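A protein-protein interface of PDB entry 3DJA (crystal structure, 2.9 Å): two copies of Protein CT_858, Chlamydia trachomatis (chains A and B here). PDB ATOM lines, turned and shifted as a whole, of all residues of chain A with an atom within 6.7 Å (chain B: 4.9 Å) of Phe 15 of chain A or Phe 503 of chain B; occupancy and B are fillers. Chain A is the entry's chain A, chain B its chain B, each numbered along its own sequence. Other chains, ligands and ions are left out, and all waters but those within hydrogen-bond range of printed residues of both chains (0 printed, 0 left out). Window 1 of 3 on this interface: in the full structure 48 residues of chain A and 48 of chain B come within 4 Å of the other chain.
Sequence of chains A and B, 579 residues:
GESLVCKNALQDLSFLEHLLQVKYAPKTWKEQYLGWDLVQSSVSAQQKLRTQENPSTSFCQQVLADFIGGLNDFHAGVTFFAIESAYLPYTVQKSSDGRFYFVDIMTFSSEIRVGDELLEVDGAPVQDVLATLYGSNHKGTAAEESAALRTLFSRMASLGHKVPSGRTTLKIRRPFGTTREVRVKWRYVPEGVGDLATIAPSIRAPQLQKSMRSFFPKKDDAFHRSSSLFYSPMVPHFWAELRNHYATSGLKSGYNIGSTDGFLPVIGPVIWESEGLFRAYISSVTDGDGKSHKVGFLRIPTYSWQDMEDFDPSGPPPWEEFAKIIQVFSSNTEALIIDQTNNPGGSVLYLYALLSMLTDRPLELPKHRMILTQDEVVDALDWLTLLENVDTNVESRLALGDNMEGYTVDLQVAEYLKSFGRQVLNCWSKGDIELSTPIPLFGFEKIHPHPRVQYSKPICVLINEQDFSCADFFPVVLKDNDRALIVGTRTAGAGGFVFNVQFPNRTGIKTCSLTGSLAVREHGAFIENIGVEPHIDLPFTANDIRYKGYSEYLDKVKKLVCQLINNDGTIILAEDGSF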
ATOM      1  N   ALA A   9     -15.977  18.135 -14.348  1.00  0.00           N
ATOM      2  CA  ALA A   9     -15.480  17.187 -15.337  1.00  0.00           C
ATOM      3  C   ALA A   9     -16.128  15.806 -15.184  1.00  0.00           C
ATOM      4  O   ALA A   9     -16.581  15.219 -16.171  1.00  0.00           O
ATOM      5  CB  ALA A   9     -13.974  17.076 -15.224  1.00  0.00           C
ATOM      6  N   LEU A  10     -16.174  15.288 -13.956  1.00  0.00           N
ATOM      7  CA  LEU A  10     -16.778  13.978 -13.711  1.00  0.00           C
ATOM      8  C   LEU A  10     -18.242  13.972 -14.103  1.00  0.00           C
ATOM      9  O   LEU A  10     -18.735  13.023 -14.719  1.00  0.00           O
ATOM     10  CB  LEU A  10     -16.639  13.594 -12.235  1.00  0.00           C
ATOM     11  CG  LEU A  10     -15.215  13.231 -11.792  1.00  0.00           C
ATOM     12  CD1 LEU A  10     -15.134  13.164 -10.278  1.00  0.00           C
ATOM     13  CD2 LEU A  10     -14.812  11.904 -12.421  1.00  0.00           C
ATOM     14  N   GLN A  11     -18.932  15.040 -13.732  1.00  0.00           N
ATOM     15  CA  GLN A  11     -20.344  15.208 -14.039  1.00  0.00           C
ATOM     16  C   GLN A  11     -20.459  15.232 -15.549  1.00  0.00           C
ATOM     17  O   GLN A  11     -21.198  14.460 -16.143  1.00  0.00           O
ATOM     18  CB  GLN A  11     -20.849  16.534 -13.464  1.00  0.00           C
ATOM     19  CG  GLN A  11     -22.167  16.450 -12.681  1.00  0.00           C
ATOM     20  CD  GLN A  11     -23.315  15.994 -13.548  1.00  0.00           C
ATOM     21  OE1 GLN A  11     -23.477  16.473 -14.672  1.00  0.00           O
ATOM     22  NE2 GLN A  11     -24.126  15.070 -13.033  1.00  0.00           N
ATOM     23  N   ASP A  12     -19.698  16.124 -16.170  1.00  0.00           N
ATOM     24  CA  ASP A  12     -19.709  16.244 -17.616  1.00  0.00           C
ATOM     25  C   ASP A  12     -19.295  14.928 -18.278  1.00  0.00           C
ATOM     26  O   ASP A  12     -19.756  14.616 -19.381  1.00  0.00           O
ATOM     27  CB  ASP A  12     -18.804  17.408 -18.039  1.00  0.00           C
ATOM     28  CG  ASP A  12     -19.392  18.785 -17.639  1.00  0.00           C
ATOM     29  OD1 ASP A  12     -20.594  19.019 -17.938  1.00  0.00           O
ATOM     30  OD2 ASP A  12     -18.675  19.631 -17.035  1.00  0.00           O
ATOM     31  N   LEU A  13     -18.458  14.144 -17.596  1.00  0.00           N
ATOM     32  CA  LEU A  13     -18.007  12.862 -18.126  1.00  0.00           C
ATOM     33  C   LEU A  13     -19.113  11.843 -18.001  1.00  0.00           C
ATOM     34  O   LEU A  13     -19.312  11.016 -18.887  1.00  0.00           O
ATOM     35  CB  LEU A  13     -16.763  12.372 -17.375  1.00  0.00           C
ATOM     36  CG  LEU A  13     -16.171  10.984 -17.683  1.00  0.00           C
ATOM     37  CD1 LEU A  13     -16.960   9.883 -16.959  1.00  0.00           C
ATOM     38  CD2 LEU A  13     -16.166  10.769 -19.191  1.00  0.00           C
ATOM     39  N   SER A  14     -19.841  11.900 -16.894  1.00  0.00           N
ATOM     40  CA  SER A  14     -20.933  10.950 -16.692  1.00  0.00           C
ATOM     41  C   SER A  14     -22.025  11.139 -17.739  1.00  0.00           C
ATOM     42  O   SER A  14     -22.662  10.172 -18.157  1.00  0.00           O
ATOM     43  CB  SER A  14     -21.519  11.078 -15.279  1.00  0.00           C
ATOM     44  OG  SER A  14     -21.902  12.411 -14.980  1.00  0.00           O
ATOM     45  N   PHE A  15     -22.224  12.383 -18.168  1.00  0.00           N
ATOM     46  CA  PHE A  15     -23.228  12.692 -19.175  1.00  0.00           C
ATOM     47  C   PHE A  15     -22.782  12.114 -20.525  1.00  0.00           C
ATOM     48  O   PHE A  15     -23.592  11.555 -21.278  1.00  0.00           O
ATOM     49  CB  PHE A  15     -23.411  14.205 -19.290  1.00  0.00           C
ATOM     50  CG  PHE A  15     -24.492  14.612 -20.247  1.00  0.00           C
ATOM     51  CD1 PHE A  15     -25.829  14.333 -19.966  1.00  0.00           C
ATOM     52  CD2 PHE A  15     -24.177  15.257 -21.434  1.00  0.00           C
ATOM     53  CE1 PHE A  15     -26.836  14.691 -20.855  1.00  0.00           C
ATOM     54  CE2 PHE A  15     -25.167  15.615 -22.326  1.00  0.00           C
ATOM     55  CZ  PHE A  15     -26.507  15.333 -22.036  1.00  0.00           C
ATOM     56  N   LEU A  16     -21.495  12.248 -20.836  1.00  0.00           N
ATOM     57  CA  LEU A  16     -20.996  11.712 -22.087  1.00  0.00           C
ATOM     58  C   LEU A  16     -21.177  10.210 -22.053  1.00  0.00           C
ATOM     59  O   LEU A  16     -21.586   9.588 -23.027  1.00  0.00           O
ATOM     60  CB  LEU A  16     -19.524  12.068 -22.274  1.00  0.00           C
ATOM     61  CG  LEU A  16     -19.242  13.536 -22.608  1.00  0.00           C
ATOM     62  CD1 LEU A  16     -17.794  13.700 -23.041  1.00  0.00           C
ATOM     63  CD2 LEU A  16     -20.172  13.989 -23.735  1.00  0.00           C
ATOM     64  N   GLU A  17     -20.888   9.625 -20.905  1.00  0.00           N
ATOM     65  CA  GLU A  17     -21.033   8.191 -20.747  1.00  0.00           C
ATOM     66  C   GLU A  17     -22.473   7.770 -21.014  1.00  0.00           C
ATOM     67  O   GLU A  17     -22.720   6.754 -21.652  1.00  0.00           O
ATOM     68  CB  GLU A  17     -20.627   7.787 -19.340  1.00  0.00           C
ATOM     69  CG  GLU A  17     -20.475   6.300 -19.170  1.00  0.00           C
ATOM     70  CD  GLU A  17     -19.631   5.947 -17.967  1.00  0.00           C
ATOM     71  OE1 GLU A  17     -19.415   4.736 -17.751  1.00  0.00           O
ATOM     72  OE2 GLU A  17     -19.184   6.878 -17.248  1.00  0.00           O
ATOM     73  N   HIS A  18     -23.428   8.559 -20.537  1.00  0.00           N
ATOM     74  CA  HIS A  18     -24.829   8.236 -20.742  1.00  0.00           C
ATOM     75  C   HIS A  18     -25.299   8.357 -22.208  1.00  0.00           C
ATOM     76  O   HIS A  18     -26.188   7.614 -22.639  1.00  0.00           O
ATOM     77  CB  HIS A  18     -25.684   9.110 -19.828  1.00  0.00           C
ATOM     78  CG  HIS A  18     -27.156   8.925 -20.017  1.00  0.00           C
ATOM     79  ND1 HIS A  18     -27.905   9.728 -20.854  1.00  0.00           N
ATOM     80  CD2 HIS A  18     -28.018   8.024 -19.486  1.00  0.00           C
ATOM     81  CE1 HIS A  18     -29.167   9.330 -20.826  1.00  0.00           C
ATOM     82  NE2 HIS A  18     -29.261   8.299 -20.004  1.00  0.00           N
ATOM     83  N   LEU A  19     -24.717   9.285 -22.970  1.00  0.00           N
ATOM     84  CA  LEU A  19     -25.093   9.446 -24.373  1.00  0.00           C
ATOM     85  C   LEU A  19     -24.678   8.186 -25.124  1.00  0.00           C
ATOM     86  O   LEU A  19     -25.399   7.689 -25.999  1.00  0.00           O
ATOM     87  CB  LEU A  19     -24.400  10.664 -24.984  1.00  0.00           C
ATOM     88  CG  LEU A  19     -24.916  12.030 -24.526  1.00  0.00           C
ATOM     89  CD1 LEU A  19     -23.968  13.154 -24.920  1.00  0.00           C
ATOM     90  CD2 LEU A  19     -26.279  12.252 -25.133  1.00  0.00           C
ATOM     91  N   LEU A  20     -23.514   7.658 -24.768  1.00  0.00           N
ATOM     92  CA  LEU A  20     -23.019   6.456 -25.413  1.00  0.00           C
ATOM     93  C   LEU A  20     -23.986   5.288 -25.233  1.00  0.00           C
ATOM     94  O   LEU A  20     -24.107   4.430 -26.115  1.00  0.00           O
ATOM     95  CB  LEU A  20     -21.643   6.095 -24.853  1.00  0.00           C
ATOM     96  CG  LEU A  20     -20.509   7.074 -25.185  1.00  0.00           C
ATOM     97  CD1 LEU A  20     -19.261   6.655 -24.434  1.00  0.00           C
ATOM     98  CD2 LEU A  20     -20.228   7.088 -26.688  1.00  0.00           C
ATOM     99  N   VAL A 501     -24.468  17.190 -30.107  1.00  0.00           N
ATOM    100  CA  VAL A 501     -25.158  17.455 -28.864  1.00  0.00           C
ATOM    101  C   VAL A 501     -24.506  18.623 -28.162  1.00  0.00           C
ATOM    102  O   VAL A 501     -23.276  18.711 -28.083  1.00  0.00           O
ATOM    103  CB  VAL A 501     -25.108  16.267 -27.911  1.00  0.00           C
ATOM    104  CG1 VAL A 501     -25.874  16.600 -26.641  1.00  0.00           C
ATOM    105  CG2 VAL A 501     -25.677  15.031 -28.576  1.00  0.00           C
ATOM    106  N   GLN A 502     -25.342  19.528 -27.663  1.00  0.00           N
ATOM    107  CA  GLN A 502     -24.873  20.701 -26.935  1.00  0.00           C
ATOM    108  C   GLN A 502     -25.595  20.736 -25.607  1.00  0.00           C
ATOM    109  O   GLN A 502     -26.697  20.220 -25.481  1.00  0.00           O
ATOM    110  CB  GLN A 502     -25.186  21.961 -27.712  1.00  0.00           C
ATOM    111  CG  GLN A 502     -24.613  21.957 -29.089  1.00  0.00           C
ATOM    112  CD  GLN A 502     -25.487  22.728 -30.030  1.00  0.00           C
ATOM    113  OE1 GLN A 502     -26.586  22.273 -30.385  1.00  0.00           O
ATOM    114  NE2 GLN A 502     -25.029  23.918 -30.432  1.00  0.00           N
ATOM    115  N   PHE A 503     -24.977  21.352 -24.614  1.00  0.00           N
ATOM    116  CA  PHE A 503     -25.584  21.441 -23.301  1.00  0.00           C
ATOM    117  C   PHE A 503     -24.688  22.309 -22.431  1.00  0.00           C
ATOM    118  O   PHE A 503     -23.462  22.239 -22.516  1.00  0.00           O
ATOM    119  CB  PHE A 503     -25.707  20.045 -22.702  1.00  0.00           C
ATOM    120  CG  PHE A 503     -24.382  19.384 -22.424  1.00  0.00           C
ATOM    121  CD1 PHE A 503     -23.746  19.566 -21.196  1.00  0.00           C
ATOM    122  CD2 PHE A 503     -23.764  18.585 -23.395  1.00  0.00           C
ATOM    123  CE1 PHE A 503     -22.508  18.962 -20.932  1.00  0.00           C
ATOM    124  CE2 PHE A 503     -22.531  17.976 -23.149  1.00  0.00           C
ATOM    125  CZ  PHE A 503     -21.901  18.164 -21.915  1.00  0.00           C
ATOM    126  N   ASP B  12     -31.663  11.516 -16.176  1.00  0.00           N
ATOM    127  CA  ASP B  12     -32.107  12.786 -16.721  1.00  0.00           C
ATOM    128  C   ASP B  12     -32.509  13.787 -15.634  1.00  0.00           C
ATOM    129  O   ASP B  12     -32.407  15.003 -15.816  1.00  0.00           O
ATOM    130  CB  ASP B  12     -33.239  12.517 -17.710  1.00  0.00           C
ATOM    131  CG  ASP B  12     -32.828  11.495 -18.777  1.00  0.00           C
ATOM    132  OD1 ASP B  12     -31.656  11.542 -19.235  1.00  0.00           O
ATOM    133  OD2 ASP B  12     -33.660  10.649 -19.162  1.00  0.00           O
ATOM    134  N   PHE B  15     -29.434  15.307 -14.487  1.00  0.00           N
ATOM    135  CA  PHE B  15     -28.909  16.255 -15.458  1.00  0.00           C
ATOM    136  C   PHE B  15     -29.620  17.607 -15.315  1.00  0.00           C
ATOM    137  O   PHE B  15     -28.968  18.667 -15.247  1.00  0.00           O
ATOM    138  CB  PHE B  15     -29.108  15.745 -16.878  1.00  0.00           C
ATOM    139  CG  PHE B  15     -28.481  16.623 -17.917  1.00  0.00           C
ATOM    140  CD1 PHE B  15     -27.103  16.851 -17.909  1.00  0.00           C
ATOM    141  CD2 PHE B  15     -29.267  17.257 -18.876  1.00  0.00           C
ATOM    142  CE1 PHE B  15     -26.518  17.696 -18.834  1.00  0.00           C
ATOM    143  CE2 PHE B  15     -28.695  18.103 -19.807  1.00  0.00           C
ATOM    144  CZ  PHE B  15     -27.311  18.326 -19.785  1.00  0.00           C
ATOM    145  N   LEU B  16     -30.953  17.574 -15.287  1.00  0.00           N
ATOM    146  CA  LEU B  16     -31.712  18.803 -15.129  1.00  0.00           C
ATOM    147  C   LEU B  16     -31.248  19.474 -13.845  1.00  0.00           C
ATOM    148  O   LEU B  16     -31.089  20.687 -13.778  1.00  0.00           O
ATOM    149  CB  LEU B  16     -33.206  18.512 -15.045  1.00  0.00           C
ATOM    150  CG  LEU B  16     -33.871  17.964 -16.306  1.00  0.00           C
ATOM    151  CD1 LEU B  16     -35.369  17.839 -16.075  1.00  0.00           C
ATOM    152  CD2 LEU B  16     -33.593  18.891 -17.492  1.00  0.00           C
ATOM    153  N   VAL B 501     -32.451  23.813 -23.882  1.00  0.00           N
ATOM    154  CA  VAL B 501     -31.505  22.714 -23.859  1.00  0.00           C
ATOM    155  C   VAL B 501     -32.161  21.454 -24.408  1.00  0.00           C
ATOM    156  O   VAL B 501     -33.242  21.062 -23.966  1.00  0.00           O
ATOM    157  CB  VAL B 501     -31.004  22.415 -22.448  1.00  0.00           C
ATOM    158  CG1 VAL B 501     -29.890  21.401 -22.530  1.00  0.00           C
ATOM    159  CG2 VAL B 501     -30.537  23.698 -21.773  1.00  0.00           C
ATOM    160  N   GLN B 502     -31.512  20.846 -25.393  1.00  0.00           N
ATOM    161  CA  GLN B 502     -31.993  19.610 -25.982  1.00  0.00           C
ATOM    162  C   GLN B 502     -30.863  18.599 -25.777  1.00  0.00           C
ATOM    163  O   GLN B 502     -29.698  18.979 -25.712  1.00  0.00           O
ATOM    164  CB  GLN B 502     -32.279  19.780 -27.480  1.00  0.00           C
ATOM    165  CG  GLN B 502     -33.259  20.883 -27.840  1.00  0.00           C
ATOM    166  CD  GLN B 502     -32.580  22.109 -28.445  1.00  0.00           C
ATOM    167  OE1 GLN B 502     -33.246  23.092 -28.767  1.00  0.00           O
ATOM    168  NE2 GLN B 502     -31.255  22.057 -28.602  1.00  0.00           N
ATOM    169  N   PHE B 503     -31.204  17.320 -25.661  1.00  0.00           N
ATOM    170  CA  PHE B 503     -30.209  16.269 -25.474  1.00  0.00           C
ATOM    171  C   PHE B 503     -30.903  14.922 -25.566  1.00  0.00           C
ATOM    172  O   PHE B 503     -31.975  14.736 -25.012  1.00  0.00           O
ATOM    173  CB  PHE B 503     -29.530  16.431 -24.121  1.00  0.00           C
ATOM    174  CG  PHE B 503     -30.447  16.248 -22.971  1.00  0.00           C
ATOM    175  CD1 PHE B 503     -30.445  15.061 -22.250  1.00  0.00           C
ATOM    176  CD2 PHE B 503     -31.341  17.250 -22.619  1.00  0.00           C
ATOM    177  CE1 PHE B 503     -31.328  14.869 -21.183  1.00  0.00           C
ATOM    178  CE2 PHE B 503     -32.230  17.072 -21.555  1.00  0.00           C
ATOM    179  CZ  PHE B 503     -32.225  15.874 -20.833  1.00  0.00           C
ATOM    180  N   PRO B 504     -30.298  13.954 -26.265  1.00  0.00           N
ATOM    181  CA  PRO B 504     -30.979  12.660 -26.361  1.00  0.00           C
ATOM    182  C   PRO B 504     -31.148  11.924 -25.040  1.00  0.00           C
ATOM    183  O   PRO B 504     -30.270  11.958 -24.170  1.00  0.00           O
ATOM    184  CB  PRO B 504     -30.121  11.893 -27.370  1.00  0.00           C
ATOM    185  CG  PRO B 504     -28.762  12.419 -27.132  1.00  0.00           C
ATOM    186  CD  PRO B 504     -28.967  13.906 -26.901  1.00  0.00           C
ATOM    187  N   ASN B 505     -32.294  11.265 -24.899  1.00  0.00           N
ATOM    188  CA  ASN B 505     -32.613  10.494 -23.702  1.00  0.00           C
ATOM    189  C   ASN B 505     -33.731   9.497 -24.006  1.00  0.00           C
ATOM    190  O   ASN B 505     -34.326   9.520 -25.084  1.00  0.00           O
ATOM    191  CB  ASN B 505     -33.043  11.423 -22.573  1.00  0.00           C
ATOM    192  CG  ASN B 505     -34.241  12.263 -22.945  1.00  0.00           C
ATOM    193  OD1 ASN B 505     -35.339  11.742 -23.131  1.00  0.00           O
ATOM    194  ND2 ASN B 505     -34.037  13.572 -23.069  1.00  0.00           N
ATOM    195  N   ILE B 509     -37.740  13.376 -22.964  1.00  0.00           N
ATOM    196  CA  ILE B 509     -37.576  14.825 -22.831  1.00  0.00           C
ATOM    197  C   ILE B 509     -37.232  15.419 -24.196  1.00  0.00           C
ATOM    198  O   ILE B 509     -36.384  14.879 -24.901  1.00  0.00           O
ATOM    199  CB  ILE B 509     -36.435  15.174 -21.874  1.00  0.00           C
ATOM    200  CG1 ILE B 509     -36.669  14.506 -20.519  1.00  0.00           C
ATOM    201  CG2 ILE B 509     -36.319  16.692 -21.733  1.00  0.00           C
ATOM    202  CD1 ILE B 509     -35.474  14.605 -19.582  1.00  0.00           C
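Of the 9 printed residues of chain B, 5 touch a printed residue of chain A. Hydrophobic or aromatic side chains of chain B within 4 Å of the printed part of chain A: Phe 15, Phe 503 and Pro 504. Printed residues of chain A that touch a printed residue of chain B: Phe 15, His 18, Leu 19, Val 501, Gln 502 and Phe 503. Among the printed residues, no Asp or Glu carboxylate lies within 4 Å of a Lys or Arg side-chain nitrogen of the other chain.
Leu 13 of chain A touches none of the printed residues of chain B. Phe 15 of chain A touches just these residues of chain B: Phe 15 (3.5 Å) and Phe 503 (3.8 Å). Of the printed residues of chain B, Val 501 of chain A touches Pro 504. Of the printed residues of chain B, Phe 503 of chain A touches Phe 15. Of the printed residues of chain A, Asp 12 of chain B touches His 18. Of the printed residues of chain A, Phe 503 of chain B touches Phe 15 (3.8 Å). Of the printed residues of chain A, Pro 504 of chain B touches Leu 19 and Val 501. The nearest residue of chain A that does not touch Phe 503 of chain B is Val 501 of chain A (4.4 Å).
The backbone carbonyl oxygen of Gln 502 of chain A sits close to the backbone carbonyl oxygen of Gln 502 of chain B, at 3.3 Å.
Among the printed residues, merely in contact across the chains: Leu 19 of chain A with Pro 504 of chain B (3.2 Å), Phe 15 of chain A with Phe 15 of chain B (3.5 Å), His 18 of chain A with Asp 12 of chain B (3.7 Å), Phe 503 of chain A with Phe 15 of chain B (3.7 Å), Phe 15 of chain A with Phe 503 of chain B (3.8 Å) and Val 501 of chain A with Pro 504 of chain B (3.9 Å).
The backbone carbonyl oxygen of Phe 503 of chain B sits at hydrogen-bond distance from the side-chain amide nitrogen of Asn 505 of chain B, 3.1 Å away.
Phe 15 of chain B touches its own counterpart, Phe 15 of chain A. Phe 15 of chain A touches Phe 503 of chain B, and with the chains exchanged Phe 503 of chain A touches Phe 15 of chain B. Gln 502 of chain B touches its own counterpart, Gln 502 of chain A. Positions printed for both chains: 12, 15, 16, 501, 502 and 503. Of the 7 pairs that touch across the chains among the printed residues, 4 have their exchanged pair printed and touching as well.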
